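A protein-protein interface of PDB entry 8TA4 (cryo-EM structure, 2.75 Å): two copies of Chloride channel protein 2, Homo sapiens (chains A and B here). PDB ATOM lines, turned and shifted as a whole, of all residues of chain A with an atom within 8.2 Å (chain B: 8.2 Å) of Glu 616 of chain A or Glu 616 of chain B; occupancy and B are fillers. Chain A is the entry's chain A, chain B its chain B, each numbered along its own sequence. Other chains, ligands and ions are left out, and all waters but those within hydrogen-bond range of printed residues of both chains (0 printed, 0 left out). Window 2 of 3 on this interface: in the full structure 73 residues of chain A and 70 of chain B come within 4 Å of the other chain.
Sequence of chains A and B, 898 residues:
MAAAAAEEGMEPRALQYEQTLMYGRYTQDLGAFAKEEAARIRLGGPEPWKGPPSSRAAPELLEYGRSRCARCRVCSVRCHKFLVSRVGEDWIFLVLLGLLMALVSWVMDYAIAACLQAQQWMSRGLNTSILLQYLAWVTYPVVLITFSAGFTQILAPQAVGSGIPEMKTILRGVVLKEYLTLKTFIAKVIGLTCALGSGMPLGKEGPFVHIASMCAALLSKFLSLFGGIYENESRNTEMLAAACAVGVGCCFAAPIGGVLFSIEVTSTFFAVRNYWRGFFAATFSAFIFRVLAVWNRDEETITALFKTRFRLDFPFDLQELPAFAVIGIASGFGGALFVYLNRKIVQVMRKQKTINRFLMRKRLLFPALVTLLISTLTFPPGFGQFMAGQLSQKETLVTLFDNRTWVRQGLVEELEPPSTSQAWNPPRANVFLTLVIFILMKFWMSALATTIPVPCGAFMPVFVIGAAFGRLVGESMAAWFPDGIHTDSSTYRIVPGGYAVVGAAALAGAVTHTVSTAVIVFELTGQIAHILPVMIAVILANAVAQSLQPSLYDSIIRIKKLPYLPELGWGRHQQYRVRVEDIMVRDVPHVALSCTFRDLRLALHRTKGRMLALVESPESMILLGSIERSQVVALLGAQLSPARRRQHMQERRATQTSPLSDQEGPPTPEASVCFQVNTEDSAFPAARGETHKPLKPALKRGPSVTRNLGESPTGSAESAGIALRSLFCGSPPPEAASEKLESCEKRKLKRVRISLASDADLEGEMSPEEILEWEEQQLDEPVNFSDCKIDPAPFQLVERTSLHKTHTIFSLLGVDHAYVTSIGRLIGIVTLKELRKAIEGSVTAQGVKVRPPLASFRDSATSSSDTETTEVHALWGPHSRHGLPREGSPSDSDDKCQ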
ATOM      1  N   HIS A 590      12.265 -25.691   1.234  1.00  0.00           N
ATOM      2  CA  HIS A 590      11.914 -24.805   2.332  1.00  0.00           C
ATOM      3  C   HIS A 590      11.760 -23.379   1.824  1.00  0.00           C
ATOM      4  O   HIS A 590      12.177 -23.043   0.714  1.00  0.00           O
ATOM      5  CB  HIS A 590      12.974 -24.847   3.430  1.00  0.00           C
ATOM      6  CG  HIS A 590      14.235 -24.129   3.069  1.00  0.00           C
ATOM      7  ND1 HIS A 590      15.168 -24.654   2.204  1.00  0.00           N
ATOM      8  CD2 HIS A 590      14.709 -22.918   3.445  1.00  0.00           C
ATOM      9  CE1 HIS A 590      16.169 -23.803   2.068  1.00  0.00           C
ATOM     10  NE2 HIS A 590      15.914 -22.742   2.811  1.00  0.00           N
ATOM     11  N   VAL A 591      11.147 -22.539   2.660  1.00  0.00           N
ATOM     12  CA  VAL A 591      11.062 -21.103   2.434  1.00  0.00           C
ATOM     13  C   VAL A 591      11.528 -20.391   3.698  1.00  0.00           C
ATOM     14  O   VAL A 591      11.533 -20.956   4.792  1.00  0.00           O
ATOM     15  CB  VAL A 591       9.639 -20.638   2.045  1.00  0.00           C
ATOM     16  CG1 VAL A 591       9.023 -21.584   1.040  1.00  0.00           C
ATOM     17  CG2 VAL A 591       8.752 -20.523   3.271  1.00  0.00           C
ATOM     18  N   ALA A 592      11.932 -19.140   3.532  1.00  0.00           N
ATOM     19  CA  ALA A 592      12.463 -18.343   4.624  1.00  0.00           C
ATOM     20  C   ALA A 592      11.404 -17.361   5.120  1.00  0.00           C
ATOM     21  O   ALA A 592      10.243 -17.397   4.703  1.00  0.00           O
ATOM     22  CB  ALA A 592      13.738 -17.630   4.178  1.00  0.00           C
ATOM     23  N   LEU A 593      11.799 -16.474   6.034  1.00  0.00           N
ATOM     24  CA  LEU A 593      10.864 -15.465   6.518  1.00  0.00           C
ATOM     25  C   LEU A 593      10.803 -14.266   5.580  1.00  0.00           C
ATOM     26  O   LEU A 593       9.736 -13.666   5.409  1.00  0.00           O
ATOM     27  CB  LEU A 593      11.243 -15.019   7.930  1.00  0.00           C
ATOM     28  CG  LEU A 593      10.518 -15.727   9.079  1.00  0.00           C
ATOM     29  CD1 LEU A 593      10.667 -14.946  10.375  1.00  0.00           C
ATOM     30  CD2 LEU A 593       9.050 -15.952   8.750  1.00  0.00           C
ATOM     31  N   SER A 594      11.933 -13.893   4.976  1.00  0.00           N
ATOM     32  CA  SER A 594      11.928 -12.834   3.972  1.00  0.00           C
ATOM     33  C   SER A 594      11.078 -13.265   2.786  1.00  0.00           C
ATOM     34  O   SER A 594      10.021 -12.678   2.532  1.00  0.00           O
ATOM     35  CB  SER A 594      13.354 -12.502   3.529  1.00  0.00           C
ATOM     36  OG  SER A 594      14.002 -13.640   2.989  1.00  0.00           O
ATOM     37  N   CYS A 595      11.538 -14.285   2.066  1.00  0.00           N
ATOM     38  CA  CYS A 595      10.728 -15.070   1.134  1.00  0.00           C
ATOM     39  C   CYS A 595       9.851 -14.199   0.236  1.00  0.00           C
ATOM     40  O   CYS A 595       8.624 -14.218   0.312  1.00  0.00           O
ATOM     41  CB  CYS A 595       9.875 -16.083   1.889  1.00  0.00           C
ATOM     42  SG  CYS A 595       9.062 -17.299   0.834  1.00  0.00           S
ATOM     43  N   ALA A 613       8.930 -26.612   4.365  1.00  0.00           N
ATOM     44  CA  ALA A 613       9.382 -26.188   5.682  1.00  0.00           C
ATOM     45  C   ALA A 613       9.623 -24.685   5.720  1.00  0.00           C
ATOM     46  O   ALA A 613       9.895 -24.050   4.700  1.00  0.00           O
ATOM     47  CB  ALA A 613      10.657 -26.928   6.072  1.00  0.00           C
ATOM     48  N   LEU A 614       9.523 -24.117   6.916  1.00  0.00           N
ATOM     49  CA  LEU A 614       9.696 -22.688   7.131  1.00  0.00           C
ATOM     50  C   LEU A 614      10.875 -22.454   8.061  1.00  0.00           C
ATOM     51  O   LEU A 614      10.977 -23.095   9.111  1.00  0.00           O
ATOM     52  CB  LEU A 614       8.431 -22.068   7.720  1.00  0.00           C
ATOM     53  CG  LEU A 614       8.527 -20.590   8.093  1.00  0.00           C
ATOM     54  CD1 LEU A 614       8.439 -19.710   6.861  1.00  0.00           C
ATOM     55  CD2 LEU A 614       7.451 -20.234   9.088  1.00  0.00           C
ATOM     56  N   VAL A 615      11.758 -21.533   7.682  1.00  0.00           N
ATOM     57  CA  VAL A 615      12.933 -21.208   8.476  1.00  0.00           C
ATOM     58  C   VAL A 615      12.949 -19.711   8.750  1.00  0.00           C
ATOM     59  O   VAL A 615      12.412 -18.911   7.978  1.00  0.00           O
ATOM     60  CB  VAL A 615      14.238 -21.653   7.783  1.00  0.00           C
ATOM     61  CG1 VAL A 615      14.216 -23.148   7.537  1.00  0.00           C
ATOM     62  CG2 VAL A 615      14.431 -20.906   6.485  1.00  0.00           C
ATOM     63  N   GLU A 616      13.574 -19.336   9.866  1.00  0.00           N
ATOM     64  CA  GLU A 616      13.590 -17.935  10.272  1.00  0.00           C
ATOM     65  C   GLU A 616      14.435 -17.085   9.330  1.00  0.00           C
ATOM     66  O   GLU A 616      14.094 -15.929   9.055  1.00  0.00           O
ATOM     67  CB  GLU A 616      14.099 -17.820  11.708  1.00  0.00           C
ATOM     68  CG  GLU A 616      15.000 -16.629  11.965  1.00  0.00           C
ATOM     69  CD  GLU A 616      15.311 -16.443  13.433  1.00  0.00           C
ATOM     70  OE1 GLU A 616      16.139 -15.569  13.760  1.00  0.00           O
ATOM     71  OE2 GLU A 616      14.728 -17.175  14.260  1.00  0.00           O
ATOM     72  N   SER A 617      15.539 -17.636   8.822  1.00  0.00           N
ATOM     73  CA  SER A 617      16.458 -16.876   7.986  1.00  0.00           C
ATOM     74  C   SER A 617      17.285 -17.853   7.175  1.00  0.00           C
ATOM     75  O   SER A 617      17.658 -18.904   7.711  1.00  0.00           O
ATOM     76  CB  SER A 617      17.370 -15.990   8.842  1.00  0.00           C
ATOM     77  OG  SER A 617      18.273 -15.243   8.047  1.00  0.00           O
ATOM     78  N   PRO A 618      17.599 -17.561   5.912  1.00  0.00           N
ATOM     79  CA  PRO A 618      18.461 -18.478   5.154  1.00  0.00           C
ATOM     80  C   PRO A 618      19.894 -18.506   5.649  1.00  0.00           C
ATOM     81  O   PRO A 618      20.630 -19.443   5.320  1.00  0.00           O
ATOM     82  CB  PRO A 618      18.357 -17.948   3.720  1.00  0.00           C
ATOM     83  CG  PRO A 618      18.104 -16.495   3.877  1.00  0.00           C
ATOM     84  CD  PRO A 618      17.459 -16.261   5.231  1.00  0.00           C
ATOM     85  N   GLU A 619      20.314 -17.513   6.433  1.00  0.00           N
ATOM     86  CA  GLU A 619      21.646 -17.555   7.025  1.00  0.00           C
ATOM     87  C   GLU A 619      21.706 -18.553   8.172  1.00  0.00           C
ATOM     88  O   GLU A 619      22.699 -19.273   8.325  1.00  0.00           O
ATOM     89  CB  GLU A 619      22.052 -16.161   7.507  1.00  0.00           C
ATOM     90  CG  GLU A 619      21.330 -14.985   6.835  1.00  0.00           C
ATOM     91  CD  GLU A 619      21.503 -14.918   5.323  1.00  0.00           C
ATOM     92  OE1 GLU A 619      22.299 -15.692   4.751  1.00  0.00           O
ATOM     93  OE2 GLU A 619      20.829 -14.075   4.697  1.00  0.00           O
ATOM     94  N   SER A 620      20.654 -18.610   8.989  1.00  0.00           N
ATOM     95  CA  SER A 620      20.603 -19.502  10.140  1.00  0.00           C
ATOM     96  C   SER A 620      19.797 -20.766   9.887  1.00  0.00           C
ATOM     97  O   SER A 620      20.142 -21.818  10.432  1.00  0.00           O
ATOM     98  CB  SER A 620      20.020 -18.768  11.352  1.00  0.00           C
ATOM     99  OG  SER A 620      18.679 -18.380  11.118  1.00  0.00           O
ATOM    100  N   MET A 621      18.741 -20.684   9.076  1.00  0.00           N
ATOM    101  CA  MET A 621      17.917 -21.840   8.713  1.00  0.00           C
ATOM    102  C   MET A 621      17.336 -22.535   9.941  1.00  0.00           C
ATOM    103  O   MET A 621      17.275 -23.763  10.007  1.00  0.00           O
ATOM    104  CB  MET A 621      18.705 -22.832   7.854  1.00  0.00           C
ATOM    105  CG  MET A 621      18.952 -22.365   6.437  1.00  0.00           C
ATOM    106  SD  MET A 621      18.008 -23.333   5.248  1.00  0.00           S
ATOM    107  CE  MET A 621      19.001 -24.817   5.152  1.00  0.00           C
ATOM    108  N   ILE A 622      16.896 -21.750  10.916  1.00  0.00           N
ATOM    109  CA  ILE A 622      16.307 -22.307  12.129  1.00  0.00           C
ATOM    110  C   ILE A 622      14.877 -22.738  11.837  1.00  0.00           C
ATOM    111  O   ILE A 622      14.059 -21.941  11.368  1.00  0.00           O
ATOM    112  CB  ILE A 622      16.366 -21.289  13.277  1.00  0.00           C
ATOM    113  CG1 ILE A 622      17.739 -21.328  13.942  1.00  0.00           C
ATOM    114  CG2 ILE A 622      15.285 -21.574  14.302  1.00  0.00           C
ATOM    115  CD1 ILE A 622      18.230 -19.979  14.392  1.00  0.00           C
ATOM    116  N   LEU A 623      14.575 -24.005  12.109  1.00  0.00           N
ATOM    117  CA  LEU A 623      13.276 -24.566  11.766  1.00  0.00           C
ATOM    118  C   LEU A 623      12.177 -23.999  12.654  1.00  0.00           C
ATOM    119  O   LEU A 623      12.345 -23.862  13.869  1.00  0.00           O
ATOM    120  CB  LEU A 623      13.314 -26.087  11.887  1.00  0.00           C
ATOM    121  CG  LEU A 623      12.054 -26.853  11.490  1.00  0.00           C
ATOM    122  CD1 LEU A 623      11.744 -26.654  10.023  1.00  0.00           C
ATOM    123  CD2 LEU A 623      12.220 -28.325  11.804  1.00  0.00           C
ATOM    124  N   LEU A 624      11.036 -23.682  12.040  1.00  0.00           N
ATOM    125  CA  LEU A 624       9.900 -23.124  12.763  1.00  0.00           C
ATOM    126  C   LEU A 624       8.652 -23.974  12.570  1.00  0.00           C
ATOM    127  O   LEU A 624       7.853 -24.133  13.497  1.00  0.00           O
ATOM    128  CB  LEU A 624       9.624 -21.691  12.310  1.00  0.00           C
ATOM    129  CG  LEU A 624      10.680 -20.639  12.633  1.00  0.00           C
ATOM    130  CD1 LEU A 624      10.179 -19.263  12.256  1.00  0.00           C
ATOM    131  CD2 LEU A 624      11.048 -20.691  14.098  1.00  0.00           C
ATOM    132  N   GLY A 625       8.472 -24.517  11.372  1.00  0.00           N
ATOM    133  CA  GLY A 625       7.297 -25.320  11.093  1.00  0.00           C
ATOM    134  C   GLY A 625       7.219 -25.662   9.620  1.00  0.00           C
ATOM    135  O   GLY A 625       8.208 -25.570   8.895  1.00  0.00           O
ATOM    136  N   ILE A 823      21.240 -28.091  15.839  1.00  0.00           N
ATOM    137  CA  ILE A 823      20.840 -27.265  16.976  1.00  0.00           C
ATOM    138  C   ILE A 823      19.465 -26.649  16.731  1.00  0.00           C
ATOM    139  O   ILE A 823      18.539 -26.843  17.518  1.00  0.00           O
ATOM    140  CB  ILE A 823      21.900 -26.181  17.285  1.00  0.00           C
ATOM    141  CG1 ILE A 823      22.919 -26.694  18.305  1.00  0.00           C
ATOM    142  CG2 ILE A 823      21.255 -24.918  17.827  1.00  0.00           C
ATOM    143  CD1 ILE A 823      23.871 -27.736  17.772  1.00  0.00           C
ATOM    144  N   GLY A 824      19.313 -25.912  15.637  1.00  0.00           N
ATOM    145  CA  GLY A 824      18.008 -25.493  15.175  1.00  0.00           C
ATOM    146  C   GLY A 824      17.961 -25.515  13.665  1.00  0.00           C
ATOM    147  O   GLY A 824      16.925 -25.234  13.061  1.00  0.00           O
ATOM    148  N   HIS B 590      16.027 -19.851  31.544  1.00  0.00           N
ATOM    149  CA  HIS B 590      16.619 -19.862  30.217  1.00  0.00           C
ATOM    150  C   HIS B 590      17.723 -18.821  30.138  1.00  0.00           C
ATOM    151  O   HIS B 590      17.788 -17.888  30.943  1.00  0.00           O
ATOM    152  CB  HIS B 590      15.572 -19.591  29.138  1.00  0.00           C
ATOM    153  CG  HIS B 590      15.171 -18.154  29.044  1.00  0.00           C
ATOM    154  ND1 HIS B 590      14.313 -17.563  29.945  1.00  0.00           N
ATOM    155  CD2 HIS B 590      15.520 -17.186  28.166  1.00  0.00           C
ATOM    156  CE1 HIS B 590      14.147 -16.294  29.622  1.00  0.00           C
ATOM    157  NE2 HIS B 590      14.871 -16.040  28.548  1.00  0.00           N
ATOM    158  N   VAL B 591      18.596 -18.996  29.146  1.00  0.00           N
ATOM    159  CA  VAL B 591      19.660 -18.051  28.841  1.00  0.00           C
ATOM    160  C   VAL B 591      19.620 -17.758  27.349  1.00  0.00           C
ATOM    161  O   VAL B 591      19.061 -18.517  26.556  1.00  0.00           O
ATOM    162  CB  VAL B 591      21.054 -18.572  29.247  1.00  0.00           C
ATOM    163  CG1 VAL B 591      21.112 -18.830  30.738  1.00  0.00           C
ATOM    164  CG2 VAL B 591      21.398 -19.829  28.472  1.00  0.00           C
ATOM    165  N   ALA B 592      20.222 -16.638  26.972  1.00  0.00           N
ATOM    166  CA  ALA B 592      20.274 -16.217  25.584  1.00  0.00           C
ATOM    167  C   ALA B 592      21.607 -16.617  24.959  1.00  0.00           C
ATOM    168  O   ALA B 592      22.494 -17.169  25.613  1.00  0.00           O
ATOM    169  CB  ALA B 592      20.048 -14.710  25.480  1.00  0.00           C
ATOM    170  N   LEU B 593      21.747 -16.331  23.663  1.00  0.00           N
ATOM    171  CA  LEU B 593      22.990 -16.640  22.966  1.00  0.00           C
ATOM    172  C   LEU B 593      24.094 -15.650  23.318  1.00  0.00           C
ATOM    173  O   LEU B 593      25.261 -16.039  23.440  1.00  0.00           O
ATOM    174  CB  LEU B 593      22.759 -16.666  21.456  1.00  0.00           C
ATOM    175  CG  LEU B 593      22.782 -18.047  20.800  1.00  0.00           C
ATOM    176  CD1 LEU B 593      22.810 -17.918  19.287  1.00  0.00           C
ATOM    177  CD2 LEU B 593      23.971 -18.861  21.291  1.00  0.00           C
ATOM    178  N   SER B 594      23.752 -14.369  23.475  1.00  0.00           N
ATOM    179  CA  SER B 594      24.743 -13.388  23.903  1.00  0.00           C
ATOM    180  C   SER B 594      25.191 -13.665  25.333  1.00  0.00           C
ATOM    181  O   SER B 594      26.354 -14.002  25.578  1.00  0.00           O
ATOM    182  CB  SER B 594      24.166 -11.977  23.778  1.00  0.00           C
ATOM    183  OG  SER B 594      22.965 -11.857  24.517  1.00  0.00           O
ATOM    184  N   CYS B 595      24.269 -13.539  26.286  1.00  0.00           N
ATOM    185  CA  CYS B 595      24.439 -14.023  27.655  1.00  0.00           C
ATOM    186  C   CYS B 595      25.738 -13.515  28.288  1.00  0.00           C
ATOM    187  O   CYS B 595      26.672 -14.270  28.550  1.00  0.00           O
ATOM    188  CB  CYS B 595      24.378 -15.551  27.695  1.00  0.00           C
ATOM    189  SG  CYS B 595      23.793 -16.217  29.267  1.00  0.00           S
ATOM    190  N   ALA B 613      17.137 -23.919  29.590  1.00  0.00           N
ATOM    191  CA  ALA B 613      16.887 -23.840  28.162  1.00  0.00           C
ATOM    192  C   ALA B 613      17.753 -22.756  27.530  1.00  0.00           C
ATOM    193  O   ALA B 613      18.203 -21.817  28.188  1.00  0.00           O
ATOM    194  CB  ALA B 613      15.411 -23.563  27.888  1.00  0.00           C
ATOM    195  N   LEU B 614      17.994 -22.904  26.232  1.00  0.00           N
ATOM    196  CA  LEU B 614      18.783 -21.956  25.461  1.00  0.00           C
ATOM    197  C   LEU B 614      17.911 -21.377  24.359  1.00  0.00           C
ATOM    198  O   LEU B 614      17.310 -22.126  23.584  1.00  0.00           O
ATOM    199  CB  LEU B 614      20.019 -22.633  24.862  1.00  0.00           C
ATOM    200  CG  LEU B 614      21.312 -21.824  24.757  1.00  0.00           C
ATOM    201  CD1 LEU B 614      22.444 -22.731  24.346  1.00  0.00           C
ATOM    202  CD2 LEU B 614      21.175 -20.676  23.776  1.00  0.00           C
ATOM    203  N   VAL B 615      17.845 -20.053  24.288  1.00  0.00           N
ATOM    204  CA  VAL B 615      17.074 -19.372  23.257  1.00  0.00           C
ATOM    205  C   VAL B 615      18.025 -18.545  22.407  1.00  0.00           C
ATOM    206  O   VAL B 615      19.085 -18.113  22.869  1.00  0.00           O
ATOM    207  CB  VAL B 615      15.958 -18.487  23.849  1.00  0.00           C
ATOM    208  CG1 VAL B 615      14.924 -19.345  24.554  1.00  0.00           C
ATOM    209  CG2 VAL B 615      16.539 -17.463  24.798  1.00  0.00           C
ATOM    210  N   GLU B 616      17.641 -18.334  21.146  1.00  0.00           N
ATOM    211  CA  GLU B 616      18.509 -17.606  20.227  1.00  0.00           C
ATOM    212  C   GLU B 616      18.729 -16.172  20.686  1.00  0.00           C
ATOM    213  O   GLU B 616      19.850 -15.655  20.615  1.00  0.00           O
ATOM    214  CB  GLU B 616      17.922 -17.629  18.816  1.00  0.00           C
ATOM    215  CG  GLU B 616      18.836 -17.022  17.771  1.00  0.00           C
ATOM    216  CD  GLU B 616      18.137 -16.787  16.450  1.00  0.00           C
ATOM    217  OE1 GLU B 616      16.900 -16.620  16.452  1.00  0.00           O
ATOM    218  OE2 GLU B 616      18.825 -16.767  15.407  1.00  0.00           O
ATOM    219  N   SER B 617      17.676 -15.512  21.158  1.00  0.00           N
ATOM    220  CA  SER B 617      17.778 -14.137  21.621  1.00  0.00           C
ATOM    221  C   SER B 617      16.605 -13.857  22.540  1.00  0.00           C
ATOM    222  O   SER B 617      15.547 -14.475  22.387  1.00  0.00           O
ATOM    223  CB  SER B 617      17.782 -13.155  20.441  1.00  0.00           C
ATOM    224  OG  SER B 617      16.690 -13.400  19.574  1.00  0.00           O
ATOM    225  N   PRO B 618      16.755 -12.946  23.504  1.00  0.00           N
ATOM    226  CA  PRO B 618      15.604 -12.577  24.342  1.00  0.00           C
ATOM    227  C   PRO B 618      14.458 -11.951  23.564  1.00  0.00           C
ATOM    228  O   PRO B 618      13.315 -11.997  24.036  1.00  0.00           O
ATOM    229  CB  PRO B 618      16.206 -11.593  25.355  1.00  0.00           C
ATOM    230  CG  PRO B 618      17.676 -11.885  25.345  1.00  0.00           C
ATOM    231  CD  PRO B 618      17.994 -12.288  23.945  1.00  0.00           C
ATOM    232  N   GLU B 619      14.721 -11.362  22.396  1.00  0.00           N
ATOM    233  CA  GLU B 619      13.641 -10.809  21.588  1.00  0.00           C
ATOM    234  C   GLU B 619      12.835 -11.902  20.897  1.00  0.00           C
ATOM    235  O   GLU B 619      11.612 -11.784  20.768  1.00  0.00           O
ATOM    236  CB  GLU B 619      14.183  -9.824  20.541  1.00  0.00           C
ATOM    237  CG  GLU B 619      15.202  -8.780  21.021  1.00  0.00           C
ATOM    238  CD  GLU B 619      16.587  -9.338  21.304  1.00  0.00           C
ATOM    239  OE1 GLU B 619      17.578  -8.690  20.906  1.00  0.00           O
ATOM    240  OE2 GLU B 619      16.693 -10.418  21.915  1.00  0.00           O
ATOM    241  N   SER B 620      13.495 -12.965  20.443  1.00  0.00           N
ATOM    242  CA  SER B 620      12.833 -13.990  19.646  1.00  0.00           C
ATOM    243  C   SER B 620      12.461 -15.233  20.439  1.00  0.00           C
ATOM    244  O   SER B 620      11.465 -15.883  20.108  1.00  0.00           O
ATOM    245  CB  SER B 620      13.721 -14.396  18.465  1.00  0.00           C
ATOM    246  OG  SER B 620      12.942 -14.947  17.419  1.00  0.00           O
ATOM    247  N   MET B 621      13.238 -15.580  21.466  1.00  0.00           N
ATOM    248  CA  MET B 621      12.934 -16.700  22.357  1.00  0.00           C
ATOM    249  C   MET B 621      12.820 -18.023  21.605  1.00  0.00           C
ATOM    250  O   MET B 621      12.018 -18.884  21.970  1.00  0.00           O
ATOM    251  CB  MET B 621      11.654 -16.439  23.154  1.00  0.00           C
ATOM    252  CG  MET B 621      11.806 -15.446  24.283  1.00  0.00           C
ATOM    253  SD  MET B 621      11.670 -16.201  25.911  1.00  0.00           S
ATOM    254  CE  MET B 621      12.334 -14.891  26.929  1.00  0.00           C
ATOM    255  N   ILE B 622      13.618 -18.210  20.560  1.00  0.00           N
ATOM    256  CA  ILE B 622      13.561 -19.439  19.775  1.00  0.00           C
ATOM    257  C   ILE B 622      14.372 -20.513  20.487  1.00  0.00           C
ATOM    258  O   ILE B 622      15.578 -20.358  20.691  1.00  0.00           O
ATOM    259  CB  ILE B 622      14.079 -19.213  18.349  1.00  0.00           C
ATOM    260  CG1 ILE B 622      13.283 -18.108  17.655  1.00  0.00           C
ATOM    261  CG2 ILE B 622      14.027 -20.507  17.559  1.00  0.00           C
ATOM    262  CD1 ILE B 622      12.084 -18.595  16.889  1.00  0.00           C
ATOM    263  N   LEU B 623      13.711 -21.608  20.851  1.00  0.00           N
ATOM    264  CA  LEU B 623      14.374 -22.684  21.576  1.00  0.00           C
ATOM    265  C   LEU B 623      15.411 -23.374  20.699  1.00  0.00           C
ATOM    266  O   LEU B 623      15.183 -23.612  19.511  1.00  0.00           O
ATOM    267  CB  LEU B 623      13.341 -23.698  22.066  1.00  0.00           C
ATOM    268  CG  LEU B 623      13.835 -24.835  22.956  1.00  0.00           C
ATOM    269  CD1 LEU B 623      14.283 -24.306  24.303  1.00  0.00           C
ATOM    270  CD2 LEU B 623      12.755 -25.883  23.123  1.00  0.00           C
ATOM    271  N   LEU B 624      16.560 -23.695  21.294  1.00  0.00           N
ATOM    272  CA  LEU B 624      17.634 -24.368  20.575  1.00  0.00           C
ATOM    273  C   LEU B 624      18.072 -25.642  21.286  1.00  0.00           C
ATOM    274  O   LEU B 624      18.453 -26.621  20.639  1.00  0.00           O
ATOM    275  CB  LEU B 624      18.838 -23.440  20.406  1.00  0.00           C
ATOM    276  CG  LEU B 624      18.630 -22.092  19.721  1.00  0.00           C
ATOM    277  CD1 LEU B 624      19.958 -21.377  19.589  1.00  0.00           C
ATOM    278  CD2 LEU B 624      17.982 -22.268  18.364  1.00  0.00           C
ATOM    279  N   GLY B 625      18.029 -25.640  22.613  1.00  0.00           N
ATOM    280  CA  GLY B 625      18.498 -26.786  23.368  1.00  0.00           C
ATOM    281  C   GLY B 625      18.515 -26.485  24.852  1.00  0.00           C
ATOM    282  O   GLY B 625      17.775 -25.627  25.331  1.00  0.00           O
ATOM    283  N   ILE B 823       5.512 -21.768  17.430  1.00  0.00           N
ATOM    284  CA  ILE B 823       6.293 -21.259  16.306  1.00  0.00           C
ATOM    285  C   ILE B 823       7.689 -20.983  16.875  1.00  0.00           C
ATOM    286  O   ILE B 823       8.229 -19.873  16.800  1.00  0.00           O
ATOM    287  CB  ILE B 823       5.584 -20.052  15.643  1.00  0.00           C
ATOM    288  CG1 ILE B 823       4.630 -20.566  14.572  1.00  0.00           C
ATOM    289  CG2 ILE B 823       6.502 -19.152  14.821  1.00  0.00           C
ATOM    290  CD1 ILE B 823       5.327 -21.213  13.398  1.00  0.00           C
ATOM    291  N   GLY B 824       8.251 -21.987  17.542  1.00  0.00           N
ATOM    292  CA  GLY B 824       9.610 -21.922  18.025  1.00  0.00           C
ATOM    293  C   GLY B 824       9.819 -21.131  19.298  1.00  0.00           C
ATOM    294  O   GLY B 824      10.885 -21.252  19.909  1.00  0.00           O
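OE1 of Glu 616 of chain A lies close to OE1 of Glu 616 of chain B (3.0 Å). O of Leu 624 of chain B lies close to O of Ile 823 of chain A (3.1 Å).
The backbone NH (N) of Leu 624 of chain A sits at hydrogen-bond distance from the backbone carbonyl oxygen (O) of Leu 614 of chain A, at 3.0 Å. The backbone NH (N) of Glu 616 of chain A lies within hydrogen-bond range of the backbone carbonyl oxygen (O) of Ile 622 of chain A, 3.0 Å away. The backbone carbonyl oxygen (O) of Leu 614 of chain B sits at hydrogen-bond distance from the backbone NH (N) of Leu 624 of chain B, 2.9 Å away. N of Glu 616 of chain B is in hydrogen-bond range of O of Ile 622 of chain B, 2.9 Å away.
Among the printed residues, merely in contact across the chains: Ile 622 of chain A with Glu 616 of chain B (3.4 Å), Leu 624 of chain A with Ile 622 of chain B (3.6 Å), Ile 622 of chain A with Ile 622 of chain B (3.7 Å), Glu 616 of chain A with Ile 622 of chain B (3.8 Å) and Leu 624 of chain A with Ile 823 of chain B (3.9 Å).
Glu 616 of chain A touches just these residues of chain B: Glu 616 (3.0 Å) and Ile 622 (3.8 Å). Of the printed residues of chain B, Leu 624 of chain A touches Ile 622 (3.6 Å) and Ile 823 (3.9 Å). Printed residues of chain A within 4 Å of Leu 624 of chain B: Ile 823 (3.1 Å). Of the printed residues of chain A, Ile 823 of chain B touches Leu 624 (3.9 Å). Ser 594 of chain B touches none of the printed residues of chain A. The nearest printed residue of chain A that does not touch Ile 823 of chain B is Leu 614 of chain A (4.9 Å).
Of the 21 printed residues of chain B, 4 touch a printed residue of chain A. Hydrophobic or aromatic side chains of chain B that line the printed part of chain A: Ile 622, Leu 624 and Ile 823. Hydrophobic or aromatic side chains of chain A that line the printed part of chain B: Ile 622, Leu 624 and Ile 823. Among the printed residues, no Asp or Glu carboxylate lies within 4 Å of a Lys or Arg side-chain nitrogen of the other chain.
Glu 616 of chain B touches its own counterpart, Glu 616 of chain A. Glu 616 of chain A touches Ile 622 of chain B, and with the chains exchanged Ile 622 of chain A touches Glu 616 of chain B. Ile 622 of chain A touches its own counterpart, Ile 622 of chain B. Leu 624 of chain A touches Ile 622 of chain B, but with the chains exchanged Ile 622 of chain A does not touch Leu 624 of chain B (4.5 Å). Positions printed for both chains: 590, 591, 592, 593, 594, 595, 613, 614, 615, 616, 617, 618, 619, 620, 621, 622, 623, 624, 625, 823 and 824.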
